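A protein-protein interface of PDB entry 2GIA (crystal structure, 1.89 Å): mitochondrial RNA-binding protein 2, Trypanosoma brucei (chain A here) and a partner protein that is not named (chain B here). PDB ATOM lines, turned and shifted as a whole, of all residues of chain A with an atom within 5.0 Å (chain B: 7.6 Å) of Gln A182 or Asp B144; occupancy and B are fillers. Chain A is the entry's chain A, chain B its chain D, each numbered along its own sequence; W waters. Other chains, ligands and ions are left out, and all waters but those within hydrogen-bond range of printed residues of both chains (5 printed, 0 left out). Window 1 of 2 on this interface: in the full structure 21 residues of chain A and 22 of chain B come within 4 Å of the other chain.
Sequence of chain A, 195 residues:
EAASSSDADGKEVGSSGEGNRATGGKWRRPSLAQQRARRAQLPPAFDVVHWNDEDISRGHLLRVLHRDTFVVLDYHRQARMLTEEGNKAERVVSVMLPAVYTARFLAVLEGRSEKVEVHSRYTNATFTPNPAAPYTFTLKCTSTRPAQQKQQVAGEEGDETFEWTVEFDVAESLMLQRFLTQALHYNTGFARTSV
Of the 10 printed residues of chain A, 5 touch a printed residue of chain B.
Hydrophobic or aromatic side chains of chain A within 4 Å of the printed part of chain B: Phe A179 and Tyr A186.
Of the 19 printed residues of chain B, 6 touch a printed residue of chain A.
Printed residues of chain B that touch a printed residue of chain A: Leu B143, Asp B144, Phe B147, Phe B149, Arg B150 and Tyr B153.
Among the printed residues, Asp or Glu carboxylates within 4 Å of a Lys or Arg side-chain nitrogen of the other chain: Arg A178 with Asp B144 (2.8 Å).
Gln A182 touches just these residues of chain B: Asp B144 and Phe B149.
Asp B144 touches two residues of chain A.
Printed residues of chain B within 4 Å of Phe A179: Phe B147 and Phe B149.
Printed residues of chain A within 4 Å of Phe B147: Arg A178 (3.9 Å) and Phe A179 (3.7 Å).
Glu B145 touches none of the printed residues of chain A.
Asn A187 touches none of the printed residues of chain B.
The nearest residue of chain B that does not touch Gln A182 is Phe B147 (4.4 Å).
The nearest printed residue of chain A that does not touch Asp B144 is Thr A181 (6.0 Å).
The nearest printed residue of chain B that does not touch Tyr A186 is Glu B145 (5.0 Å).
NE of Arg A178 is in salt-bridge range of OD1 of Asp B144 (2.8 Å).
Water W2 bridges the side-chain hydroxyl of Tyr B153 (2.5 Å) and the side-chain amide oxygen of Asn A187 (2.5 Å).
Water W3 lies within hydrogen-bond range of NZ of Lys B82 (2.5 Å), OE1 of Glu B140 (2.7 Å) and NE of Arg A178 (3.4 Å).
Water W5 lies within hydrogen-bond range of the side-chain hydroxyl of Tyr A186 (2.7 Å), the side-chain amide oxygen of Gln A182 (2.8 Å) and the side-chain carboxylate of Glu B145 (3.1 Å).
Water W4 bridges OD2 of Asp B144 (2.8 Å) and NH2 of Arg A178 (3.3 Å).
Water W1 lies within hydrogen-bond range of OD1 of Asp B144, O of Glu B140 and NE of Arg A178.
The backbone carbonyl oxygen of Leu B143 lies within hydrogen-bond range of the side-chain hydroxyl of Ser B146 (2.6 Å).
The guanidinium group (NH2) of Arg B150 is in salt-bridge range of the side-chain carboxylate (OE2) of Glu B145.
Leu B143 touches Arg A178 (CD2 to CG, 3.8 Å).
Phe B147 touches Arg A178 (CE2 to C, 3.9 Å).
Phe B147 touches Phe A179 (CD1 to CD2, 3.7 Å).
Phe A179 touches Phe B149 (CE2 to CZ, 3.6 Å).
Gln A182 touches Asp B144 (OE1 to O, 3.6 Å).
Gln A182 touches Phe B149.
Phe B149 touches Ala A183.
Tyr A186 touches Phe B149.
Tyr A186 touches Arg B150 (OH to CB, 3.4 Å).
Tyr A186 touches Tyr B153.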
ATOM      1  N   ARG A 178     -20.773  14.345  -3.551  1.00  0.00           N
ATOM      2  CA  ARG A 178     -21.400  15.132  -2.472  1.00  0.00           C
ATOM      3  C   ARG A 178     -22.875  14.785  -2.379  1.00  0.00           C
ATOM      4  O   ARG A 178     -23.431  14.696  -1.293  1.00  0.00           O
ATOM      5  CB  ARG A 178     -21.232  16.646  -2.729  1.00  0.00           C
ATOM      6  CG  ARG A 178     -19.737  17.112  -2.710  1.00  0.00           C
ATOM      7  CD  ARG A 178     -18.864  16.462  -1.621  1.00  0.00           C
ATOM      8  NE  ARG A 178     -19.343  16.710  -0.248  1.00  0.00           N
ATOM      9  CZ  ARG A 178     -19.041  15.966   0.826  1.00  0.00           C
ATOM     10  NH1 ARG A 178     -18.267  14.872   0.733  1.00  0.00           N
ATOM     11  NH2 ARG A 178     -19.412  16.379   2.035  1.00  0.00           N
ATOM     12  N   PHE A 179     -23.508  14.578  -3.524  1.00  0.00           N
ATOM     13  CA  PHE A 179     -24.938  14.230  -3.544  1.00  0.00           C
ATOM     14  C   PHE A 179     -25.196  12.898  -2.835  1.00  0.00           C
ATOM     15  O   PHE A 179     -26.089  12.810  -1.997  1.00  0.00           O
ATOM     16  CB  PHE A 179     -25.441  14.153  -5.005  1.00  0.00           C
ATOM     17  CG  PHE A 179     -26.895  13.775  -5.117  1.00  0.00           C
ATOM     18  CD1 PHE A 179     -27.254  12.435  -5.329  1.00  0.00           C
ATOM     19  CD2 PHE A 179     -27.883  14.731  -5.004  1.00  0.00           C
ATOM     20  CE1 PHE A 179     -28.614  12.069  -5.410  1.00  0.00           C
ATOM     21  CE2 PHE A 179     -29.251  14.360  -5.093  1.00  0.00           C
ATOM     22  CZ  PHE A 179     -29.585  13.041  -5.296  1.00  0.00           C
ATOM     23  N   LEU A 180     -24.411  11.858  -3.169  1.00  0.00           N
ATOM     24  CA  LEU A 180     -24.599  10.555  -2.533  1.00  0.00           C
ATOM     25  C   LEU A 180     -24.250  10.633  -1.041  1.00  0.00           C
ATOM     26  O   LEU A 180     -24.864   9.941  -0.216  1.00  0.00           O
ATOM     27  CB  LEU A 180     -23.719   9.500  -3.205  1.00  0.00           C
ATOM     28  CG  LEU A 180     -24.124   9.278  -4.683  1.00  0.00           C
ATOM     29  CD1 LEU A 180     -23.151   8.329  -5.329  1.00  0.00           C
ATOM     30  CD2 LEU A 180     -25.555   8.729  -4.747  1.00  0.00           C
ATOM     31  N   THR A 181     -23.231  11.446  -0.714  1.00  0.00           N
ATOM     32  CA  THR A 181     -22.852  11.671   0.703  1.00  0.00           C
ATOM     33  C   THR A 181     -24.049  12.232   1.444  1.00  0.00           C
ATOM     34  O   THR A 181     -24.337  11.795   2.564  1.00  0.00           O
ATOM     35  CB  THR A 181     -21.657  12.637   0.794  1.00  0.00           C
ATOM     36  OG1 THR A 181     -20.535  11.959   0.258  1.00  0.00           O
ATOM     37  CG2 THR A 181     -21.325  13.086   2.298  1.00  0.00           C
ATOM     38  N   GLN A 182     -24.724  13.244   0.872  1.00  0.00           N
ATOM     39  CA  GLN A 182     -25.928  13.819   1.513  1.00  0.00           C
ATOM     40  C   GLN A 182     -27.070  12.772   1.531  1.00  0.00           C
ATOM     41  O   GLN A 182     -27.778  12.631   2.543  1.00  0.00           O
ATOM     42  CB  GLN A 182     -26.420  15.103   0.749  1.00  0.00           C
ATOM     43  CG  GLN A 182     -25.455  16.275   0.853  1.00  0.00           C
ATOM     44  CD  GLN A 182     -25.414  16.862   2.266  1.00  0.00           C
ATOM     45  OE1 GLN A 182     -26.400  17.411   2.755  1.00  0.00           O
ATOM     46  NE2 GLN A 182     -24.277  16.746   2.907  1.00  0.00           N
ATOM     47  N   ALA A 183     -27.249  12.031   0.439  1.00  0.00           N
ATOM     48  CA  ALA A 183     -28.313  11.016   0.443  1.00  0.00           C
ATOM     49  C   ALA A 183     -28.124  10.001   1.585  1.00  0.00           C
ATOM     50  O   ALA A 183     -29.093   9.658   2.309  1.00  0.00           O
ATOM     51  CB  ALA A 183     -28.371  10.273  -0.908  1.00  0.00           C
ATOM     52  N   LEU A 184     -26.887   9.541   1.777  1.00  0.00           N
ATOM     53  CA  LEU A 184     -26.610   8.567   2.834  1.00  0.00           C
ATOM     54  C   LEU A 184     -26.840   9.201   4.216  1.00  0.00           C
ATOM     55  O   LEU A 184     -27.365   8.566   5.126  1.00  0.00           O
ATOM     56  CB  LEU A 184     -25.140   8.119   2.806  1.00  0.00           C
ATOM     57  CG  LEU A 184     -24.729   6.662   2.800  1.00  0.00           C
ATOM     58  CD1 LEU A 184     -23.243   6.585   3.138  1.00  0.00           C
ATOM     59  CD2 LEU A 184     -25.608   5.833   3.720  1.00  0.00           C
ATOM     60  N   HIS A 185     -26.411  10.444   4.375  1.00  0.00           N
ATOM     61  CA  HIS A 185     -26.577  11.160   5.663  1.00  0.00           C
ATOM     62  C   HIS A 185     -28.065  11.245   6.032  1.00  0.00           C
ATOM     63  O   HIS A 185     -28.482  10.898   7.147  1.00  0.00           O
ATOM     64  CB  HIS A 185     -26.023  12.598   5.522  1.00  0.00           C
ATOM     65  CG  HIS A 185     -25.936  13.361   6.818  1.00  0.00           C
ATOM     66  ND1 HIS A 185     -24.878  13.208   7.690  1.00  0.00           N
ATOM     67  CD2 HIS A 185     -26.730  14.312   7.355  1.00  0.00           C
ATOM     68  CE1 HIS A 185     -25.017  14.047   8.700  1.00  0.00           C
ATOM     69  NE2 HIS A 185     -26.136  14.726   8.527  1.00  0.00           N
ATOM     70  N   TYR A 186     -28.875  11.725   5.106  1.00  0.00           N
ATOM     71  CA  TYR A 186     -30.291  11.884   5.399  1.00  0.00           C
ATOM     72  C   TYR A 186     -30.999  10.550   5.483  1.00  0.00           C
ATOM     73  O   TYR A 186     -31.841  10.347   6.375  1.00  0.00           O
ATOM     74  CB  TYR A 186     -30.980  12.778   4.349  1.00  0.00           C
ATOM     75  CG  TYR A 186     -30.708  14.252   4.576  1.00  0.00           C
ATOM     76  CD1 TYR A 186     -31.649  15.064   5.206  1.00  0.00           C
ATOM     77  CD2 TYR A 186     -29.481  14.795   4.255  1.00  0.00           C
ATOM     78  CE1 TYR A 186     -31.364  16.394   5.518  1.00  0.00           C
ATOM     79  CE2 TYR A 186     -29.159  16.153   4.597  1.00  0.00           C
ATOM     80  CZ  TYR A 186     -30.119  16.926   5.230  1.00  0.00           C
ATOM     81  OH  TYR A 186     -29.829  18.195   5.675  1.00  0.00           O
ATOM     82  N   ASN A 187     -30.673   9.635   4.579  1.00  0.00           N
ATOM     83  CA  ASN A 187     -31.346   8.336   4.638  1.00  0.00           C
ATOM     84  C   ASN A 187     -31.048   7.567   5.905  1.00  0.00           C
ATOM     85  O   ASN A 187     -31.863   6.767   6.353  1.00  0.00           O
ATOM     86  CB  ASN A 187     -30.981   7.454   3.436  1.00  0.00           C
ATOM     87  CG  ASN A 187     -32.029   6.374   3.199  1.00  0.00           C
ATOM     88  OD1 ASN A 187     -33.194   6.687   2.960  1.00  0.00           O
ATOM     89  ND2 ASN A 187     -31.631   5.106   3.281  1.00  0.00           N
ATOM     90  N   HIS B  71     -24.351  25.893 -11.471  1.00  0.00           N
ATOM     91  CA  HIS B  71     -24.155  24.874 -10.447  1.00  0.00           C
ATOM     92  C   HIS B  71     -22.841  24.107 -10.698  1.00  0.00           C
ATOM     93  O   HIS B  71     -22.072  23.838  -9.766  1.00  0.00           O
ATOM     94  CB  HIS B  71     -25.394  23.934 -10.460  1.00  0.00           C
ATOM     95  CG  HIS B  71     -25.443  22.923  -9.344  1.00  0.00           C
ATOM     96  ND1 HIS B  71     -24.926  23.153  -8.081  1.00  0.00           N
ATOM     97  CD2 HIS B  71     -26.104  21.738  -9.261  1.00  0.00           C
ATOM     98  CE1 HIS B  71     -25.277  22.163  -7.270  1.00  0.00           C
ATOM     99  NE2 HIS B  71     -25.997  21.295  -7.964  1.00  0.00           N
ATOM    100  N   LEU B  74     -19.767  25.893  -9.392  1.00  0.00           N
ATOM    101  CA  LEU B  74     -19.566  25.785  -7.947  1.00  0.00           C
ATOM    102  C   LEU B  74     -18.772  24.466  -7.695  1.00  0.00           C
ATOM    103  O   LEU B  74     -17.786  24.435  -6.916  1.00  0.00           O
ATOM    104  CB  LEU B  74     -20.933  25.768  -7.214  1.00  0.00           C
ATOM    105  CG  LEU B  74     -20.965  25.376  -5.725  1.00  0.00           C
ATOM    106  CD1 LEU B  74     -20.028  26.308  -4.886  1.00  0.00           C
ATOM    107  CD2 LEU B  74     -22.420  25.498  -5.214  1.00  0.00           C
ATOM    108  N   VAL B  78     -14.945  24.046  -6.044  1.00  0.00           N
ATOM    109  CA  VAL B  78     -14.575  23.148  -4.969  1.00  0.00           C
ATOM    110  C   VAL B  78     -13.450  22.213  -5.478  1.00  0.00           C
ATOM    111  O   VAL B  78     -12.515  21.904  -4.741  1.00  0.00           O
ATOM    112  CB  VAL B  78     -15.820  22.326  -4.506  1.00  0.00           C
ATOM    113  CG1 VAL B  78     -15.420  21.195  -3.539  1.00  0.00           C
ATOM    114  CG2 VAL B  78     -16.799  23.299  -3.809  1.00  0.00           C
ATOM    115  N   LYS B  82      -9.874  21.498  -3.682  1.00  0.00           N
ATOM    116  CA  LYS B  82      -9.405  20.144  -3.345  1.00  0.00           C
ATOM    117  C   LYS B  82      -8.234  19.676  -4.195  1.00  0.00           C
ATOM    118  O   LYS B  82      -7.759  18.555  -4.048  1.00  0.00           O
ATOM    119  CB  LYS B  82     -10.564  19.140  -3.482  1.00  0.00           C
ATOM    120  CG  LYS B  82     -11.635  19.380  -2.457  1.00  0.00           C
ATOM    121  CD  LYS B  82     -12.681  18.256  -2.470  1.00  0.00           C
ATOM    122  CE  LYS B  82     -13.550  18.309  -1.208  1.00  0.00           C
ATOM    123  NZ  LYS B  82     -14.929  17.793  -1.472  1.00  0.00           N
ATOM    124  N   PHE B 138     -16.967  28.050   2.684  1.00  0.00           N
ATOM    125  CA  PHE B 138     -18.223  28.552   2.102  1.00  0.00           C
ATOM    126  C   PHE B 138     -18.591  27.738   0.848  1.00  0.00           C
ATOM    127  O   PHE B 138     -19.754  27.314   0.655  1.00  0.00           O
ATOM    128  CB  PHE B 138     -18.086  30.050   1.727  1.00  0.00           C
ATOM    129  CG  PHE B 138     -19.373  30.651   1.208  1.00  0.00           C
ATOM    130  CD1 PHE B 138     -19.697  30.569  -0.137  1.00  0.00           C
ATOM    131  CD2 PHE B 138     -20.294  31.189   2.080  1.00  0.00           C
ATOM    132  CE1 PHE B 138     -20.946  31.005  -0.608  1.00  0.00           C
ATOM    133  CE2 PHE B 138     -21.540  31.627   1.632  1.00  0.00           C
ATOM    134  CZ  PHE B 138     -21.861  31.530   0.271  1.00  0.00           C
ATOM    135  N   LEU B 139     -17.604  27.522  -0.019  1.00  0.00           N
ATOM    136  CA  LEU B 139     -17.889  26.749  -1.239  1.00  0.00           C
ATOM    137  C   LEU B 139     -18.279  25.304  -0.899  1.00  0.00           C
ATOM    138  O   LEU B 139     -19.166  24.722  -1.541  1.00  0.00           O
ATOM    139  CB  LEU B 139     -16.658  26.743  -2.166  1.00  0.00           C
ATOM    140  CG  LEU B 139     -16.212  28.111  -2.729  1.00  0.00           C
ATOM    141  CD1 LEU B 139     -14.872  27.952  -3.423  1.00  0.00           C
ATOM    142  CD2 LEU B 139     -17.259  28.610  -3.717  1.00  0.00           C
ATOM    143  N   GLU B 140     -17.592  24.679   0.058  1.00  0.00           N
ATOM    144  CA  GLU B 140     -17.976  23.289   0.364  1.00  0.00           C
ATOM    145  C   GLU B 140     -19.382  23.202   0.928  1.00  0.00           C
ATOM    146  O   GLU B 140     -20.150  22.294   0.579  1.00  0.00           O
ATOM    147  CB  GLU B 140     -16.964  22.652   1.322  1.00  0.00           C
ATOM    148  CG  GLU B 140     -15.647  22.471   0.610  1.00  0.00           C
ATOM    149  CD  GLU B 140     -14.718  21.538   1.341  1.00  0.00           C
ATOM    150  OE1 GLU B 140     -15.074  20.350   1.514  1.00  0.00           O
ATOM    151  OE2 GLU B 140     -13.638  21.998   1.747  1.00  0.00           O
ATOM    152  N   SER B 141     -19.697  24.121   1.849  1.00  0.00           N
ATOM    153  CA  SER B 141     -21.047  24.221   2.450  1.00  0.00           C
ATOM    154  C   SER B 141     -22.102  24.450   1.365  1.00  0.00           C
ATOM    155  O   SER B 141     -23.191  23.826   1.354  1.00  0.00           O
ATOM    156  CB  SER B 141     -21.139  25.445   3.411  1.00  0.00           C
ATOM    157  OG  SER B 141     -20.578  25.149   4.696  1.00  0.00           O
ATOM    158  N   ALA B 142     -21.828  25.415   0.501  1.00  0.00           N
ATOM    159  CA  ALA B 142     -22.749  25.766  -0.570  1.00  0.00           C
ATOM    160  C   ALA B 142     -23.025  24.549  -1.455  1.00  0.00           C
ATOM    161  O   ALA B 142     -24.183  24.259  -1.775  1.00  0.00           O
ATOM    162  CB  ALA B 142     -22.168  26.864  -1.447  1.00  0.00           C
ATOM    163  N   LEU B 143     -21.962  23.853  -1.849  1.00  0.00           N
ATOM    164  CA  LEU B 143     -22.144  22.681  -2.726  1.00  0.00           C
ATOM    165  C   LEU B 143     -22.983  21.592  -2.004  1.00  0.00           C
ATOM    166  O   LEU B 143     -23.932  21.025  -2.584  1.00  0.00           O
ATOM    167  CB  LEU B 143     -20.770  22.142  -3.215  1.00  0.00           C
ATOM    168  CG  LEU B 143     -20.785  20.812  -4.054  1.00  0.00           C
ATOM    169  CD1 LEU B 143     -21.662  21.023  -5.298  1.00  0.00           C
ATOM    170  CD2 LEU B 143     -19.389  20.410  -4.545  1.00  0.00           C
ATOM    171  N   ASP B 144     -22.690  21.332  -0.726  1.00  0.00           N
ATOM    172  CA  ASP B 144     -23.459  20.312   0.003  1.00  0.00           C
ATOM    173  C   ASP B 144     -24.938  20.658   0.164  1.00  0.00           C
ATOM    174  O   ASP B 144     -25.813  19.782   0.110  1.00  0.00           O
ATOM    175  CB  ASP B 144     -22.854  20.063   1.390  1.00  0.00           C
ATOM    176  CG  ASP B 144     -21.592  19.232   1.317  1.00  0.00           C
ATOM    177  OD1 ASP B 144     -21.226  18.747   0.210  1.00  0.00           O
ATOM    178  OD2 ASP B 144     -20.944  19.071   2.352  1.00  0.00           O
ATOM    179  N   GLU B 145     -25.225  21.941   0.363  1.00  0.00           N
ATOM    180  CA  GLU B 145     -26.603  22.384   0.550  1.00  0.00           C
ATOM    181  C   GLU B 145     -27.306  22.692  -0.756  1.00  0.00           C
ATOM    182  O   GLU B 145     -28.491  23.021  -0.751  1.00  0.00           O
ATOM    183  CB  GLU B 145     -26.640  23.683   1.407  1.00  0.00           C
ATOM    184  CG  GLU B 145     -26.082  23.501   2.868  1.00  0.00           C
ATOM    185  CD  GLU B 145     -26.886  22.534   3.758  1.00  0.00           C
ATOM    186  OE1 GLU B 145     -28.103  22.319   3.540  1.00  0.00           O
ATOM    187  OE2 GLU B 145     -26.293  21.981   4.711  1.00  0.00           O
ATOM    188  N   SER B 146     -26.599  22.600  -1.867  1.00  0.00           N
ATOM    189  CA  SER B 146     -27.202  22.949  -3.153  1.00  0.00           C
ATOM    190  C   SER B 146     -28.245  21.979  -3.749  1.00  0.00           C
ATOM    191  O   SER B 146     -28.914  22.342  -4.679  1.00  0.00           O
ATOM    192  CB  SER B 146     -26.115  23.121  -4.213  1.00  0.00           C
ATOM    193  OG  SER B 146     -25.494  21.885  -4.523  1.00  0.00           O
ATOM    194  N   PHE B 147     -28.375  20.774  -3.215  1.00  0.00           N
ATOM    195  CA  PHE B 147     -29.265  19.776  -3.802  1.00  0.00           C
ATOM    196  C   PHE B 147     -30.677  19.826  -3.275  1.00  0.00           C
ATOM    197  O   PHE B 147     -31.592  19.287  -3.899  1.00  0.00           O
ATOM    198  CB  PHE B 147     -28.652  18.367  -3.562  1.00  0.00           C
ATOM    199  CG  PHE B 147     -27.210  18.256  -4.027  1.00  0.00           C
ATOM    200  CD1 PHE B 147     -26.899  18.228  -5.379  1.00  0.00           C
ATOM    201  CD2 PHE B 147     -26.190  18.136  -3.114  1.00  0.00           C
ATOM    202  CE1 PHE B 147     -25.562  18.070  -5.827  1.00  0.00           C
ATOM    203  CE2 PHE B 147     -24.858  17.983  -3.507  1.00  0.00           C
ATOM    204  CZ  PHE B 147     -24.519  17.945  -4.864  1.00  0.00           C
ATOM    205  N   GLY B 148     -30.822  20.440  -2.110  1.00  0.00           N
ATOM    206  CA  GLY B 148     -32.114  20.588  -1.480  1.00  0.00           C
ATOM    207  C   GLY B 148     -32.506  19.603  -0.407  1.00  0.00           C
ATOM    208  O   GLY B 148     -33.672  19.599   0.027  1.00  0.00           O
ATOM    209  N   PHE B 149     -31.563  18.791   0.081  1.00  0.00           N
ATOM    210  CA  PHE B 149     -31.925  17.805   1.096  1.00  0.00           C
ATOM    211  C   PHE B 149     -32.516  18.394   2.358  1.00  0.00           C
ATOM    212  O   PHE B 149     -33.540  17.905   2.860  1.00  0.00           O
ATOM    213  CB  PHE B 149     -30.697  16.951   1.489  1.00  0.00           C
ATOM    214  CG  PHE B 149     -30.328  15.911   0.430  1.00  0.00           C
ATOM    215  CD1 PHE B 149     -30.941  14.652   0.430  1.00  0.00           C
ATOM    216  CD2 PHE B 149     -29.394  16.216  -0.568  1.00  0.00           C
ATOM    217  CE1 PHE B 149     -30.625  13.697  -0.565  1.00  0.00           C
ATOM    218  CE2 PHE B 149     -29.062  15.291  -1.564  1.00  0.00           C
ATOM    219  CZ  PHE B 149     -29.677  14.022  -1.570  1.00  0.00           C
ATOM    220  N   ARG B 150     -31.890  19.451   2.875  1.00  0.00           N
ATOM    221  CA  ARG B 150     -32.342  19.996   4.166  1.00  0.00           C
ATOM    222  C   ARG B 150     -33.759  20.531   4.102  1.00  0.00           C
ATOM    223  O   ARG B 150     -34.587  20.220   4.957  1.00  0.00           O
ATOM    224  CB  ARG B 150     -31.372  21.075   4.663  1.00  0.00           C
ATOM    225  CG  ARG B 150     -31.628  21.548   6.128  1.00  0.00           C
ATOM    226  CD  ARG B 150     -30.688  22.743   6.461  1.00  0.00           C
ATOM    227  NE  ARG B 150     -29.267  22.360   6.439  1.00  0.00           N
ATOM    228  CZ  ARG B 150     -28.590  21.981   7.518  1.00  0.00           C
ATOM    229  NH1 ARG B 150     -29.203  21.936   8.711  1.00  0.00           N
ATOM    230  NH2 ARG B 150     -27.302  21.653   7.417  1.00  0.00           N
ATOM    231  N   GLN B 151     -34.060  21.285   3.061  1.00  0.00           N
ATOM    232  CA  GLN B 151     -35.413  21.839   2.909  1.00  0.00           C
ATOM    233  C   GLN B 151     -36.429  20.747   2.591  1.00  0.00           C
ATOM    234  O   GLN B 151     -37.555  20.762   3.114  1.00  0.00           O
ATOM    235  CB  GLN B 151     -35.457  22.882   1.793  1.00  0.00           C
ATOM    236  CG  GLN B 151     -34.542  24.082   1.971  1.00  0.00           C
ATOM    237  CD  GLN B 151     -33.037  23.737   1.948  1.00  0.00           C
ATOM    238  OE1 GLN B 151     -32.585  22.828   1.222  1.00  0.00           O
ATOM    239  NE2 GLN B 151     -32.256  24.490   2.742  1.00  0.00           N
ATOM    240  N   TYR B 153     -36.385  17.578   3.460  1.00  0.00           N
ATOM    241  CA  TYR B 153     -36.667  16.793   4.651  1.00  0.00           C
ATOM    242  C   TYR B 153     -37.317  17.570   5.777  1.00  0.00           C
ATOM    243  O   TYR B 153     -37.888  16.976   6.686  1.00  0.00           O
ATOM    244  CB  TYR B 153     -35.388  16.118   5.150  1.00  0.00           C
ATOM    245  CG  TYR B 153     -35.096  14.819   4.452  1.00  0.00           C
ATOM    246  CD1 TYR B 153     -35.280  13.611   5.130  1.00  0.00           C
ATOM    247  CD2 TYR B 153     -34.636  14.781   3.113  1.00  0.00           C
ATOM    248  CE1 TYR B 153     -35.024  12.408   4.524  1.00  0.00           C
ATOM    249  CE2 TYR B 153     -34.372  13.569   2.482  1.00  0.00           C
ATOM    250  CZ  TYR B 153     -34.570  12.380   3.210  1.00  0.00           C
ATOM    251  OH  TYR B 153     -34.294  11.152   2.681  1.00  0.00           O
HETATM  252  O   HOH W   1     -18.962  20.039  -0.812  1.00  0.00           O
HETATM  253  O   HOH W   2     -34.706   8.724   2.931  1.00  0.00           O
HETATM  254  O   HOH W   3     -16.729  18.842  -0.039  1.00  0.00           O
HETATM  255  O   HOH W   4     -18.302  19.258   3.157  1.00  0.00           O
HETATM  256  O   HOH W   5     -27.720  19.241   4.419  1.00  0.00           O
